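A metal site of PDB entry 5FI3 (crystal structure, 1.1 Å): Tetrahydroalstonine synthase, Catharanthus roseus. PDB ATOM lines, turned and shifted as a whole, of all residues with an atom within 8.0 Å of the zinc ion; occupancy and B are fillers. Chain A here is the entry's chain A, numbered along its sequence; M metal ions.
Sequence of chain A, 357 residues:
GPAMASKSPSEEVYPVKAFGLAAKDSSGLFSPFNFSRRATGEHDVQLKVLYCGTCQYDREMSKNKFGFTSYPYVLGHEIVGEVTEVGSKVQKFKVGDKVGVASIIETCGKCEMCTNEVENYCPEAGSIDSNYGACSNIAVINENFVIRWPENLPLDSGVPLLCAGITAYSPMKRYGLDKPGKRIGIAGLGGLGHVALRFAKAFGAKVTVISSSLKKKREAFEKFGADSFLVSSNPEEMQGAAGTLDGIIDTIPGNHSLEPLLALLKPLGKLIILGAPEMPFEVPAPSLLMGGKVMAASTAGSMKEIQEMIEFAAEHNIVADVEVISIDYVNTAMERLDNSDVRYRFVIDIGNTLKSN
O of Cys 111 sits at hydrogen-bond distance from OG1 of Thr 115.
The side-chain sulfur (SG) of Cys 114 sits close to the side-chain hydroxyl (OG1) of Thr 107 (3.2 Å).
The side-chain sulfur (SG) of Cys 111 sits close to the backbone NH (N) of Met 113.
N of Lys 110 sits close to SG of Cys 108, 3.4 Å away.
The side-chain sulfur (SG) of Cys 114 sits close to the backbone NH (N) of Gly 109.
The side-chain sulfur (SG) of Cys 122 sits close to the backbone NH (N) of Glu 124.
The side-chain sulfur (SG) of Cys 122 sits close to the backbone NH (N) of Ala 125 (3.7 Å).
Merely in contact with the zinc ion: Gly 109.
The nearest printed residue that does not touch the zinc ion is Lys 110 (4.4 Å).
The zinc ion is bound by the side-chain sulfur (SG) of Cys 111 (2.3 Å), the side-chain sulfur (SG) of Cys 122 (2.3 Å), the side-chain sulfur (SG) of Cys 108 (2.3 Å) and the side-chain sulfur (SG) of Cys 114 (2.4 Å).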
ATOM      1  N   GLU A 106     -21.257  -7.395   8.927  1.00  0.00           N
ATOM      2  CA  GLU A 106     -21.803  -7.713  10.240  1.00  0.00           C
ATOM      3  C   GLU A 106     -20.663  -7.712  11.241  1.00  0.00           C
ATOM      4  O   GLU A 106     -19.578  -8.152  10.908  1.00  0.00           O
ATOM      5  CB  GLU A 106     -22.487  -9.091  10.209  1.00  0.00           C
ATOM      6  CG  GLU A 106     -23.276  -9.465  11.466  1.00  0.00           C
ATOM      7  CD  GLU A 106     -24.112 -10.729  11.304  1.00  0.00           C
ATOM      8  OE1 GLU A 106     -23.898 -11.500  10.336  1.00  0.00           O
ATOM      9  OE2 GLU A 106     -25.006 -10.945  12.159  1.00  0.00           O
ATOM     10  N   THR A 107     -20.903  -7.174  12.428  1.00  0.00           N
ATOM     11  CA  THR A 107     -19.944  -7.210  13.509  1.00  0.00           C
ATOM     12  C   THR A 107     -20.706  -7.432  14.822  1.00  0.00           C
ATOM     13  O   THR A 107     -21.935  -7.435  14.832  1.00  0.00           O
ATOM     14  CB  THR A 107     -19.076  -5.955  13.574  1.00  0.00           C
ATOM     15  OG1 THR A 107     -19.858  -4.844  13.973  1.00  0.00           O
ATOM     16  CG2 THR A 107     -18.354  -5.675  12.280  1.00  0.00           C
ATOM     17  N   CYS A 108     -19.991  -7.595  15.929  1.00  0.00           N
ATOM     18  CA  CYS A 108     -20.693  -7.902  17.168  1.00  0.00           C
ATOM     19  C   CYS A 108     -21.474  -6.724  17.714  1.00  0.00           C
ATOM     20  O   CYS A 108     -22.492  -6.920  18.395  1.00  0.00           O
ATOM     21  CB  CYS A 108     -19.726  -8.463  18.209  1.00  0.00           C
ATOM     22  SG  CYS A 108     -18.776  -7.271  19.213  1.00  0.00           S
ATOM     23  N   GLY A 109     -21.018  -5.518  17.438  1.00  0.00           N
ATOM     24  CA  GLY A 109     -21.693  -4.279  17.836  1.00  0.00           C
ATOM     25  C   GLY A 109     -21.439  -3.794  19.255  1.00  0.00           C
ATOM     26  O   GLY A 109     -21.881  -2.711  19.603  1.00  0.00           O
ATOM     27  N   LYS A 110     -20.675  -4.557  20.038  1.00  0.00           N
ATOM     28  CA  LYS A 110     -20.556  -4.306  21.471  1.00  0.00           C
ATOM     29  C   LYS A 110     -19.144  -4.287  22.035  1.00  0.00           C
ATOM     30  O   LYS A 110     -18.956  -3.865  23.163  1.00  0.00           O
ATOM     31  CB  LYS A 110     -21.445  -5.306  22.183  1.00  0.00           C
ATOM     32  CG  LYS A 110     -20.785  -6.609  22.619  1.00  0.00           C
ATOM     33  N   CYS A 111     -18.145  -4.719  21.268  1.00  0.00           N
ATOM     34  CA  CYS A 111     -16.762  -4.702  21.715  1.00  0.00           C
ATOM     35  C   CYS A 111     -16.137  -3.331  21.571  1.00  0.00           C
ATOM     36  O   CYS A 111     -16.756  -2.388  20.986  1.00  0.00           O
ATOM     37  CB  CYS A 111     -15.977  -5.767  20.962  1.00  0.00           C
ATOM     38  SG  CYS A 111     -15.584  -5.303  19.262  1.00  0.00           S
ATOM     39  N   GLU A 112     -14.909  -3.210  22.067  1.00  0.00           N
ATOM     40  CA  GLU A 112     -14.218  -1.945  21.997  1.00  0.00           C
ATOM     41  C   GLU A 112     -14.070  -1.449  20.550  1.00  0.00           C
ATOM     42  O   GLU A 112     -14.196  -0.253  20.267  1.00  0.00           O
ATOM     43  CB  GLU A 112     -12.841  -2.100  22.681  1.00  0.00           C
ATOM     44  CG  GLU A 112     -11.987  -0.831  22.630  1.00  0.00           C
ATOM     45  CD  GLU A 112     -10.649  -0.976  23.323  1.00  0.00           C
ATOM     46  OE1 GLU A 112     -10.353  -2.055  23.870  1.00  0.00           O
ATOM     47  OE2 GLU A 112      -9.840  -0.020  23.269  1.00  0.00           O
ATOM     48  N   MET A 113     -13.743  -2.354  19.638  1.00  0.00           N
ATOM     49  CA  MET A 113     -13.548  -1.941  18.254  1.00  0.00           C
ATOM     50  C   MET A 113     -14.868  -1.469  17.614  1.00  0.00           C
ATOM     51  O   MET A 113     -14.898  -0.463  16.902  1.00  0.00           O
ATOM     52  CB  MET A 113     -12.916  -3.051  17.439  1.00  0.00           C
ATOM     53  CG  MET A 113     -11.578  -3.556  17.973  1.00  0.00           C
ATOM     54  SD  MET A 113     -10.321  -2.265  18.062  1.00  0.00           S
ATOM     55  CE  MET A 113      -9.490  -2.638  19.581  1.00  0.00           C
ATOM     56  N   CYS A 114     -15.950  -2.172  17.912  1.00  0.00           N
ATOM     57  CA  CYS A 114     -17.242  -1.780  17.385  1.00  0.00           C
ATOM     58  C   CYS A 114     -17.718  -0.441  17.928  1.00  0.00           C
ATOM     59  O   CYS A 114     -18.159   0.434  17.180  1.00  0.00           O
ATOM     60  CB  CYS A 114     -18.250  -2.903  17.627  1.00  0.00           C
ATOM     61  SG  CYS A 114     -18.020  -4.340  16.573  1.00  0.00           S
ATOM     62  N   THR A 115     -17.615  -0.275  19.242  1.00  0.00           N
ATOM     63  CA  THR A 115     -18.123   0.940  19.898  1.00  0.00           C
ATOM     64  C   THR A 115     -17.266   2.161  19.570  1.00  0.00           C
ATOM     65  O   THR A 115     -17.757   3.275  19.595  1.00  0.00           O
ATOM     66  CB  THR A 115     -18.325   0.770  21.398  1.00  0.00           C
ATOM     67  OG1 THR A 115     -17.080   0.485  22.008  1.00  0.00           O
ATOM     68  CG2 THR A 115     -19.277  -0.368  21.737  1.00  0.00           C
ATOM     69  N   VAL A 118     -14.396   1.448  14.770  1.00  0.00           N
ATOM     70  CA  VAL A 118     -13.371   0.752  14.010  1.00  0.00           C
ATOM     71  C   VAL A 118     -13.759  -0.722  13.926  1.00  0.00           C
ATOM     72  O   VAL A 118     -12.982  -1.617  14.149  1.00  0.00           O
ATOM     73  CB  VAL A 118     -11.938   1.008  14.519  1.00  0.00           C
ATOM     74  CG1 VAL A 118     -11.562   2.467  14.305  1.00  0.00           C
ATOM     75  CG2 VAL A 118     -11.772   0.629  15.980  1.00  0.00           C
ATOM     76  N   GLU A 119     -15.017  -0.930  13.508  1.00  0.00           N
ATOM     77  CA  GLU A 119     -15.625  -2.246  13.589  1.00  0.00           C
ATOM     78  C   GLU A 119     -15.063  -3.265  12.629  1.00  0.00           C
ATOM     79  O   GLU A 119     -15.273  -4.461  12.795  1.00  0.00           O
ATOM     80  CB  GLU A 119     -17.142  -2.188  13.475  1.00  0.00           C
ATOM     81  CG  GLU A 119     -17.660  -1.902  12.068  1.00  0.00           C
ATOM     82  CD  GLU A 119     -17.403  -0.496  11.568  1.00  0.00           C
ATOM     83  OE1 GLU A 119     -17.348   0.448  12.387  1.00  0.00           O
ATOM     84  OE2 GLU A 119     -17.288  -0.360  10.349  1.00  0.00           O
ATOM     85  N   ASN A 120     -14.320  -2.809  11.620  1.00  0.00           N
ATOM     86  CA  ASN A 120     -13.603  -3.753  10.777  1.00  0.00           C
ATOM     87  C   ASN A 120     -12.585  -4.573  11.558  1.00  0.00           C
ATOM     88  O   ASN A 120     -12.169  -5.621  11.059  1.00  0.00           O
ATOM     89  CB  ASN A 120     -12.958  -3.040   9.583  1.00  0.00           C
ATOM     90  CG  ASN A 120     -11.946  -1.993  10.008  1.00  0.00           C
ATOM     91  OD1 ASN A 120     -12.288  -1.063  10.751  1.00  0.00           O
ATOM     92  ND2 ASN A 120     -10.725  -2.097   9.494  1.00  0.00           N
ATOM     93  N   TYR A 121     -12.198  -4.104  12.741  1.00  0.00           N
ATOM     94  CA  TYR A 121     -11.299  -4.868  13.625  1.00  0.00           C
ATOM     95  C   TYR A 121     -12.026  -5.613  14.706  1.00  0.00           C
ATOM     96  O   TYR A 121     -11.382  -6.181  15.582  1.00  0.00           O
ATOM     97  CB  TYR A 121     -10.222  -3.914  14.211  1.00  0.00           C
ATOM     98  CG  TYR A 121      -9.269  -3.446  13.126  1.00  0.00           C
ATOM     99  CD1 TYR A 121      -8.442  -4.370  12.485  1.00  0.00           C
ATOM    100  CD2 TYR A 121      -9.207  -2.126  12.722  1.00  0.00           C
ATOM    101  CE1 TYR A 121      -7.599  -3.978  11.477  1.00  0.00           C
ATOM    102  CE2 TYR A 121      -8.345  -1.716  11.729  1.00  0.00           C
ATOM    103  CZ  TYR A 121      -7.558  -2.648  11.101  1.00  0.00           C
ATOM    104  OH  TYR A 121      -6.692  -2.299  10.083  1.00  0.00           O
ATOM    105  N   CYS A 122     -13.343  -5.688  14.653  1.00  0.00           N
ATOM    106  CA  CYS A 122     -14.094  -6.561  15.555  1.00  0.00           C
ATOM    107  C   CYS A 122     -13.560  -7.963  15.439  1.00  0.00           C
ATOM    108  O   CYS A 122     -13.484  -8.487  14.328  1.00  0.00           O
ATOM    109  CB  CYS A 122     -15.571  -6.570  15.164  1.00  0.00           C
ATOM    110  SG  CYS A 122     -16.555  -7.660  16.210  1.00  0.00           S
ATOM    111  N   PRO A 123     -13.145  -8.596  16.553  1.00  0.00           N
ATOM    112  CA  PRO A 123     -12.724  -9.982  16.423  1.00  0.00           C
ATOM    113  C   PRO A 123     -13.771 -10.924  15.805  1.00  0.00           C
ATOM    114  O   PRO A 123     -13.405 -11.975  15.268  1.00  0.00           O
ATOM    115  CB  PRO A 123     -12.400 -10.374  17.862  1.00  0.00           C
ATOM    116  CG  PRO A 123     -12.120  -9.089  18.584  1.00  0.00           C
ATOM    117  CD  PRO A 123     -12.968  -8.062  17.908  1.00  0.00           C
ATOM    118  N   GLU A 124     -15.063 -10.556  15.850  1.00  0.00           N
ATOM    119  CA  GLU A 124     -16.153 -11.336  15.248  1.00  0.00           C
ATOM    120  C   GLU A 124     -16.732 -10.708  13.975  1.00  0.00           C
ATOM    121  O   GLU A 124     -17.885 -10.964  13.599  1.00  0.00           O
ATOM    122  CB  GLU A 124     -17.285 -11.503  16.270  1.00  0.00           C
ATOM    123  CG  GLU A 124     -16.791 -11.932  17.642  1.00  0.00           C
ATOM    124  N   ALA A 125     -15.949  -9.861  13.289  1.00  0.00           N
ATOM    125  CA  ALA A 125     -16.415  -9.228  12.064  1.00  0.00           C
ATOM    126  C   ALA A 125     -16.720 -10.315  11.061  1.00  0.00           C
ATOM    127  O   ALA A 125     -15.985 -11.298  10.950  1.00  0.00           O
ATOM    128  CB  ALA A 125     -15.367  -8.284  11.498  1.00  0.00           C
HETATM  129 ZN    ZN M   1     -17.233  -6.158  17.860  1.00  0.00          ZN
